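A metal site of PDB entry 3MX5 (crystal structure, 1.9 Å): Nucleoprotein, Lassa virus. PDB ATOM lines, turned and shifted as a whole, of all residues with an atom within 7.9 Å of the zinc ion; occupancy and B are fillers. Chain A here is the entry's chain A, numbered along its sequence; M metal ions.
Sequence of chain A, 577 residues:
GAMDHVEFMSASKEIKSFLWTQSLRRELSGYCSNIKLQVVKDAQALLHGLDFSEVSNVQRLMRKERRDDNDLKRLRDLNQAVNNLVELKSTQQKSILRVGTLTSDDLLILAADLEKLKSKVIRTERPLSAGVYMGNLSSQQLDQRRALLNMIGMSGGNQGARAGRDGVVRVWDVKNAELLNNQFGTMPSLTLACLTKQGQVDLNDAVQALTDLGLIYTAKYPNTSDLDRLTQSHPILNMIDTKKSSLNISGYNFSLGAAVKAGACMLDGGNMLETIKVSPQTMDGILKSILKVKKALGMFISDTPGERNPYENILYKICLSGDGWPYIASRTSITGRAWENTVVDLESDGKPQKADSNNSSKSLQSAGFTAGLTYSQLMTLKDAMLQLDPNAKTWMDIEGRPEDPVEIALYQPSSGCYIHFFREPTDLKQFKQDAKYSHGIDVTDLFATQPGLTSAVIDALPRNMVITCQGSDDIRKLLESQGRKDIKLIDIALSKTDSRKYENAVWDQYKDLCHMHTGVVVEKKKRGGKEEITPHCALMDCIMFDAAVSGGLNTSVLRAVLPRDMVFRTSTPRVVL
The side-chain carboxylate (OE2) of Glu 407 sits close to a ring nitrogen (NE2) of His 420 (2.8 Å). OE1 of Glu 407 lies within hydrogen-bond range of N of Ala 538 (2.9 Å). N of Glu 399 lies within hydrogen-bond range of O of Glu 407. ND1 of His 517 sits close to O of His 536 (3.5 Å). A ring nitrogen (ND1) of His 517 lies within hydrogen-bond range of the backbone carbonyl oxygen (O) of His 439 (2.9 Å). The side-chain sulfur of Cys 537 lies close to the backbone NH of Leu 539, 3.3 Å away. SG of Cys 537 lies close to N of Met 540, 3.6 Å away. The backbone NH (N) of Met 516 sits close to the side-chain sulfur (SG) of Cys 514 (3.6 Å).
Merely in contact with the zinc ion: His 420. Five residues have an atom within 4 Å of the zinc ion: Glu 407, His 420, Cys 514, His 517 and Cys 537. The nearest printed residue that does not touch the zinc ion is Ala 538 (4.5 Å).
The zinc ion is bound by OE2 of Glu 407 (1.9 Å), NE2 of His 517 (2.0 Å), SG of Cys 537 (2.2 Å) and SG of Cys 514 (2.3 Å).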
ATOM      1  N   GLU A 399      27.407 -13.065  29.770  1.00  0.00           N
ATOM      2  CA  GLU A 399      28.109 -14.169  30.452  1.00  0.00           C
ATOM      3  C   GLU A 399      29.521 -14.245  29.879  1.00  0.00           C
ATOM      4  O   GLU A 399      29.721 -14.014  28.691  1.00  0.00           O
ATOM      5  CB  GLU A 399      27.336 -15.496  30.308  1.00  0.00           C
ATOM      6  CG  GLU A 399      26.167 -15.612  31.273  1.00  0.00           C
ATOM      7  CD  GLU A 399      26.615 -15.584  32.724  1.00  0.00           C
ATOM      8  OE1 GLU A 399      27.494 -16.396  33.098  1.00  0.00           O
ATOM      9  OE2 GLU A 399      26.135 -14.710  33.480  1.00  0.00           O
ATOM     10  N   GLU A 407      28.252 -14.893  25.951  1.00  0.00           N
ATOM     11  CA  GLU A 407      26.796 -14.753  25.781  1.00  0.00           C
ATOM     12  C   GLU A 407      26.293 -13.343  26.093  1.00  0.00           C
ATOM     13  O   GLU A 407      26.445 -12.843  27.204  1.00  0.00           O
ATOM     14  CB  GLU A 407      26.008 -15.830  26.555  1.00  0.00           C
ATOM     15  CG  GLU A 407      24.476 -15.824  26.311  1.00  0.00           C
ATOM     16  CD  GLU A 407      23.713 -16.766  27.256  1.00  0.00           C
ATOM     17  OE1 GLU A 407      24.103 -16.877  28.443  1.00  0.00           O
ATOM     18  OE2 GLU A 407      22.712 -17.388  26.827  1.00  0.00           O
ATOM     19  N   ILE A 408      25.712 -12.695  25.089  1.00  0.00           N
ATOM     20  CA  ILE A 408      25.163 -11.352  25.232  1.00  0.00           C
ATOM     21  C   ILE A 408      23.660 -11.269  24.947  1.00  0.00           C
ATOM     22  O   ILE A 408      23.127 -11.915  24.006  1.00  0.00           O
ATOM     23  CB  ILE A 408      25.835 -10.313  24.274  1.00  0.00           C
ATOM     24  CG1 ILE A 408      27.337 -10.523  24.143  1.00  0.00           C
ATOM     25  CG2 ILE A 408      25.489  -8.900  24.713  1.00  0.00           C
ATOM     26  CD1 ILE A 408      28.100 -10.274  25.366  1.00  0.00           C
ATOM     27  N   ALA A 409      22.975 -10.471  25.759  1.00  0.00           N
ATOM     28  CA  ALA A 409      21.535 -10.317  25.593  1.00  0.00           C
ATOM     29  C   ALA A 409      21.063  -8.933  26.004  1.00  0.00           C
ATOM     30  O   ALA A 409      21.513  -8.389  27.017  1.00  0.00           O
ATOM     31  CB  ALA A 409      20.758 -11.427  26.416  1.00  0.00           C
ATOM     32  N   HIS A 420      19.815 -11.773  21.357  1.00  0.00           N
ATOM     33  CA  HIS A 420      20.585 -12.785  22.099  1.00  0.00           C
ATOM     34  C   HIS A 420      21.534 -13.467  21.111  1.00  0.00           C
ATOM     35  O   HIS A 420      21.107 -13.849  20.042  1.00  0.00           O
ATOM     36  CB  HIS A 420      19.593 -13.786  22.724  1.00  0.00           C
ATOM     37  CG  HIS A 420      20.222 -14.962  23.424  1.00  0.00           C
ATOM     38  ND1 HIS A 420      19.625 -16.202  23.421  1.00  0.00           N
ATOM     39  CD2 HIS A 420      21.350 -15.086  24.156  1.00  0.00           C
ATOM     40  CE1 HIS A 420      20.362 -17.044  24.125  1.00  0.00           C
ATOM     41  NE2 HIS A 420      21.406 -16.386  24.592  1.00  0.00           N
ATOM     42  N   PHE A 421      22.813 -13.597  21.475  1.00  0.00           N
ATOM     43  CA  PHE A 421      23.833 -14.259  20.644  1.00  0.00           C
ATOM     44  C   PHE A 421      25.027 -14.700  21.467  1.00  0.00           C
ATOM     45  O   PHE A 421      25.128 -14.406  22.684  1.00  0.00           O
ATOM     46  CB  PHE A 421      24.288 -13.348  19.464  1.00  0.00           C
ATOM     47  CG  PHE A 421      24.860 -12.030  19.905  1.00  0.00           C
ATOM     48  CD1 PHE A 421      26.233 -11.860  20.107  1.00  0.00           C
ATOM     49  CD2 PHE A 421      24.005 -10.950  20.147  1.00  0.00           C
ATOM     50  CE1 PHE A 421      26.751 -10.611  20.501  1.00  0.00           C
ATOM     51  CE2 PHE A 421      24.511  -9.694  20.561  1.00  0.00           C
ATOM     52  CZ  PHE A 421      25.909  -9.536  20.737  1.00  0.00           C
ATOM     53  N   PHE A 422      25.908 -15.444  20.832  1.00  0.00           N
ATOM     54  CA  PHE A 422      27.055 -16.017  21.504  1.00  0.00           C
ATOM     55  C   PHE A 422      28.372 -15.575  20.883  1.00  0.00           C
ATOM     56  O   PHE A 422      28.385 -14.956  19.839  1.00  0.00           O
ATOM     57  CB  PHE A 422      26.906 -17.531  21.511  1.00  0.00           C
ATOM     58  CG  PHE A 422      25.552 -18.001  21.949  1.00  0.00           C
ATOM     59  CD1 PHE A 422      25.258 -18.189  23.285  1.00  0.00           C
ATOM     60  CD2 PHE A 422      24.552 -18.243  21.004  1.00  0.00           C
ATOM     61  CE1 PHE A 422      24.001 -18.635  23.693  1.00  0.00           C
ATOM     62  CE2 PHE A 422      23.273 -18.689  21.404  1.00  0.00           C
ATOM     63  CZ  PHE A 422      22.998 -18.869  22.753  1.00  0.00           C
ATOM     64  N   HIS A 439      27.836 -20.381  33.970  1.00  0.00           N
ATOM     65  CA  HIS A 439      26.994 -20.572  32.791  1.00  0.00           C
ATOM     66  C   HIS A 439      26.828 -21.994  32.251  1.00  0.00           C
ATOM     67  O   HIS A 439      25.908 -22.251  31.462  1.00  0.00           O
ATOM     68  CB  HIS A 439      27.411 -19.604  31.658  1.00  0.00           C
ATOM     69  CG  HIS A 439      28.841 -19.729  31.244  1.00  0.00           C
ATOM     70  ND1 HIS A 439      29.368 -20.883  30.731  1.00  0.00           N
ATOM     71  CD2 HIS A 439      29.836 -18.807  31.177  1.00  0.00           C
ATOM     72  CE1 HIS A 439      30.633 -20.700  30.389  1.00  0.00           C
ATOM     73  NE2 HIS A 439      30.937 -19.442  30.653  1.00  0.00           N
ATOM     74  N   ILE A 441      28.167 -23.565  29.905  1.00  0.00           N
ATOM     75  CA  ILE A 441      28.176 -23.686  28.462  1.00  0.00           C
ATOM     76  C   ILE A 441      29.353 -24.563  28.089  1.00  0.00           C
ATOM     77  O   ILE A 441      30.431 -24.396  28.647  1.00  0.00           O
ATOM     78  CB  ILE A 441      28.347 -22.324  27.771  1.00  0.00           C
ATOM     79  CG1 ILE A 441      27.282 -21.327  28.286  1.00  0.00           C
ATOM     80  CG2 ILE A 441      28.357 -22.488  26.249  1.00  0.00           C
ATOM     81  CD1 ILE A 441      27.466 -19.928  27.739  1.00  0.00           C
ATOM     82  N   TRP A 507      12.476 -19.483  33.842  1.00  0.00           N
ATOM     83  CA  TRP A 507      12.857 -20.721  33.109  1.00  0.00           C
ATOM     84  C   TRP A 507      11.602 -21.502  32.727  1.00  0.00           C
ATOM     85  O   TRP A 507      11.515 -21.977  31.606  1.00  0.00           O
ATOM     86  CB  TRP A 507      13.845 -21.593  33.884  1.00  0.00           C
ATOM     87  CG  TRP A 507      15.267 -21.038  33.929  1.00  0.00           C
ATOM     88  CD1 TRP A 507      15.841 -20.350  34.950  1.00  0.00           C
ATOM     89  CD2 TRP A 507      16.247 -21.098  32.887  1.00  0.00           C
ATOM     90  NE1 TRP A 507      17.139 -19.996  34.630  1.00  0.00           N
ATOM     91  CE2 TRP A 507      17.404 -20.436  33.357  1.00  0.00           C
ATOM     92  CE3 TRP A 507      16.269 -21.665  31.606  1.00  0.00           C
ATOM     93  CZ2 TRP A 507      18.582 -20.302  32.597  1.00  0.00           C
ATOM     94  CZ3 TRP A 507      17.439 -21.542  30.840  1.00  0.00           C
ATOM     95  CH2 TRP A 507      18.585 -20.876  31.353  1.00  0.00           C
ATOM     96  N   LEU A 513      13.721 -20.718  24.734  1.00  0.00           N
ATOM     97  CA  LEU A 513      14.432 -19.582  24.127  1.00  0.00           C
ATOM     98  C   LEU A 513      15.974 -19.660  24.283  1.00  0.00           C
ATOM     99  O   LEU A 513      16.680 -18.893  23.638  1.00  0.00           O
ATOM    100  CB  LEU A 513      13.944 -18.239  24.709  1.00  0.00           C
ATOM    101  CG  LEU A 513      12.479 -17.828  24.514  1.00  0.00           C
ATOM    102  CD1 LEU A 513      12.338 -16.306  24.797  1.00  0.00           C
ATOM    103  CD2 LEU A 513      11.971 -18.208  23.134  1.00  0.00           C
ATOM    104  N   CYS A 514      16.501 -20.523  25.142  1.00  0.00           N
ATOM    105  CA  CYS A 514      17.977 -20.772  25.174  1.00  0.00           C
ATOM    106  C   CYS A 514      18.381 -22.232  25.463  1.00  0.00           C
ATOM    107  O   CYS A 514      18.033 -22.781  26.470  1.00  0.00           O
ATOM    108  CB  CYS A 514      18.710 -19.819  26.105  1.00  0.00           C
ATOM    109  SG  CYS A 514      20.526 -20.024  26.055  1.00  0.00           S
ATOM    110  N   HIS A 515      19.130 -22.864  24.553  1.00  0.00           N
ATOM    111  CA  HIS A 515      19.469 -24.282  24.811  1.00  0.00           C
ATOM    112  C   HIS A 515      20.962 -24.504  25.090  1.00  0.00           C
ATOM    113  O   HIS A 515      21.477 -25.633  24.903  1.00  0.00           O
ATOM    114  CB  HIS A 515      19.026 -25.142  23.608  1.00  0.00           C
ATOM    115  CG  HIS A 515      17.547 -25.205  23.391  1.00  0.00           C
ATOM    116  ND1 HIS A 515      16.786 -26.294  23.759  1.00  0.00           N
ATOM    117  CD2 HIS A 515      16.683 -24.316  22.833  1.00  0.00           C
ATOM    118  CE1 HIS A 515      15.518 -26.059  23.464  1.00  0.00           C
ATOM    119  NE2 HIS A 515      15.428 -24.859  22.906  1.00  0.00           N
ATOM    120  N   MET A 516      21.659 -23.433  25.484  1.00  0.00           N
ATOM    121  CA  MET A 516      23.120 -23.360  25.454  1.00  0.00           C
ATOM    122  C   MET A 516      23.787 -23.863  26.744  1.00  0.00           C
ATOM    123  O   MET A 516      24.999 -24.099  26.794  1.00  0.00           O
ATOM    124  CB  MET A 516      23.576 -21.918  25.060  1.00  0.00           C
ATOM    125  CG  MET A 516      25.077 -21.793  24.663  1.00  0.00           C
ATOM    126  SD  MET A 516      25.704 -22.947  23.393  1.00  0.00           S
ATOM    127  CE  MET A 516      25.001 -22.343  21.848  1.00  0.00           C
ATOM    128  N   HIS A 517      22.982 -24.106  27.764  1.00  0.00           N
ATOM    129  CA  HIS A 517      23.469 -24.216  29.126  1.00  0.00           C
ATOM    130  C   HIS A 517      23.247 -25.664  29.586  1.00  0.00           C
ATOM    131  O   HIS A 517      22.153 -26.025  30.064  1.00  0.00           O
ATOM    132  CB  HIS A 517      22.729 -23.196  30.013  1.00  0.00           C
ATOM    133  CG  HIS A 517      22.859 -21.791  29.507  1.00  0.00           C
ATOM    134  ND1 HIS A 517      23.857 -20.953  29.935  1.00  0.00           N
ATOM    135  CD2 HIS A 517      22.119 -21.090  28.611  1.00  0.00           C
ATOM    136  CE1 HIS A 517      23.742 -19.778  29.316  1.00  0.00           C
ATOM    137  NE2 HIS A 517      22.689 -19.838  28.518  1.00  0.00           N
ATOM    138  N   PRO A 535      22.022 -22.900  36.017  1.00  0.00           N
ATOM    139  CA  PRO A 535      23.006 -22.123  35.243  1.00  0.00           C
ATOM    140  C   PRO A 535      22.521 -20.708  34.966  1.00  0.00           C
ATOM    141  O   PRO A 535      21.321 -20.472  34.938  1.00  0.00           O
ATOM    142  CB  PRO A 535      23.079 -22.865  33.907  1.00  0.00           C
ATOM    143  CG  PRO A 535      22.623 -24.275  34.224  1.00  0.00           C
ATOM    144  CD  PRO A 535      21.623 -24.148  35.340  1.00  0.00           C
ATOM    145  N   HIS A 536      23.445 -19.770  34.730  1.00  0.00           N
ATOM    146  CA  HIS A 536      23.101 -18.369  34.475  1.00  0.00           C
ATOM    147  C   HIS A 536      23.173 -18.112  32.977  1.00  0.00           C
ATOM    148  O   HIS A 536      24.193 -18.420  32.323  1.00  0.00           O
ATOM    149  CB  HIS A 536      24.124 -17.458  35.179  1.00  0.00           C
ATOM    150  CG  HIS A 536      24.077 -17.518  36.680  1.00  0.00           C
ATOM    151  ND1 HIS A 536      24.777 -16.638  37.472  1.00  0.00           N
ATOM    152  CD2 HIS A 536      23.396 -18.325  37.526  1.00  0.00           C
ATOM    153  CE1 HIS A 536      24.560 -16.912  38.745  1.00  0.00           C
ATOM    154  NE2 HIS A 536      23.717 -17.924  38.803  1.00  0.00           N
ATOM    155  N   CYS A 537      22.095 -17.555  32.439  1.00  0.00           N
ATOM    156  CA  CYS A 537      21.992 -17.232  31.025  1.00  0.00           C
ATOM    157  C   CYS A 537      21.754 -15.724  30.928  1.00  0.00           C
ATOM    158  O   CYS A 537      20.847 -15.203  31.614  1.00  0.00           O
ATOM    159  CB  CYS A 537      20.782 -17.965  30.458  1.00  0.00           C
ATOM    160  SG  CYS A 537      20.166 -17.376  28.846  1.00  0.00           S
ATOM    161  N   ALA A 538      22.543 -15.033  30.090  1.00  0.00           N
ATOM    162  CA  ALA A 538      22.332 -13.586  29.860  1.00  0.00           C
ATOM    163  C   ALA A 538      20.859 -13.255  29.613  1.00  0.00           C
ATOM    164  O   ALA A 538      20.397 -12.249  30.110  1.00  0.00           O
ATOM    165  CB  ALA A 538      23.179 -13.069  28.745  1.00  0.00           C
ATOM    166  N   LEU A 539      20.144 -14.085  28.834  1.00  0.00           N
ATOM    167  CA  LEU A 539      18.760 -13.747  28.474  1.00  0.00           C
ATOM    168  C   LEU A 539      17.822 -13.852  29.653  1.00  0.00           C
ATOM    169  O   LEU A 539      17.129 -12.888  29.977  1.00  0.00           O
ATOM    170  CB  LEU A 539      18.216 -14.578  27.313  1.00  0.00           C
ATOM    171  CG  LEU A 539      16.833 -14.113  26.781  1.00  0.00           C
ATOM    172  CD1 LEU A 539      16.831 -12.689  26.231  1.00  0.00           C
ATOM    173  CD2 LEU A 539      16.323 -15.088  25.724  1.00  0.00           C
ATOM    174  N   MET A 540      17.816 -15.004  30.314  1.00  0.00           N
ATOM    175  CA  MET A 540      16.955 -15.229  31.443  1.00  0.00           C
ATOM    176  C   MET A 540      17.270 -14.231  32.547  1.00  0.00           C
ATOM    177  O   MET A 540      16.393 -13.841  33.286  1.00  0.00           O
ATOM    178  CB  MET A 540      17.107 -16.670  31.936  1.00  0.00           C
ATOM    179  CG  MET A 540      16.951 -17.680  30.753  1.00  0.00           C
ATOM    180  SD  MET A 540      15.334 -17.428  29.969  1.00  0.00           S
ATOM    181  CE  MET A 540      15.722 -17.780  28.262  1.00  0.00           C
ATOM    182  N   ASP A 541      18.528 -13.790  32.614  1.00  0.00           N
ATOM    183  CA  ASP A 541      18.960 -12.837  33.636  1.00  0.00           C
ATOM    184  C   ASP A 541      18.319 -11.457  33.432  1.00  0.00           C
ATOM    185  O   ASP A 541      17.849 -10.841  34.404  1.00  0.00           O
ATOM    186  CB  ASP A 541      20.470 -12.784  33.704  1.00  0.00           C
ATOM    187  CG  ASP A 541      21.050 -13.702  34.796  1.00  0.00           C
ATOM    188  OD1 ASP A 541      20.305 -14.481  35.442  1.00  0.00           O
ATOM    189  OD2 ASP A 541      22.248 -13.642  35.011  1.00  0.00           O
HETATM  190 ZN    ZN M   1      21.422 -18.605  27.594  1.00  0.00          ZN
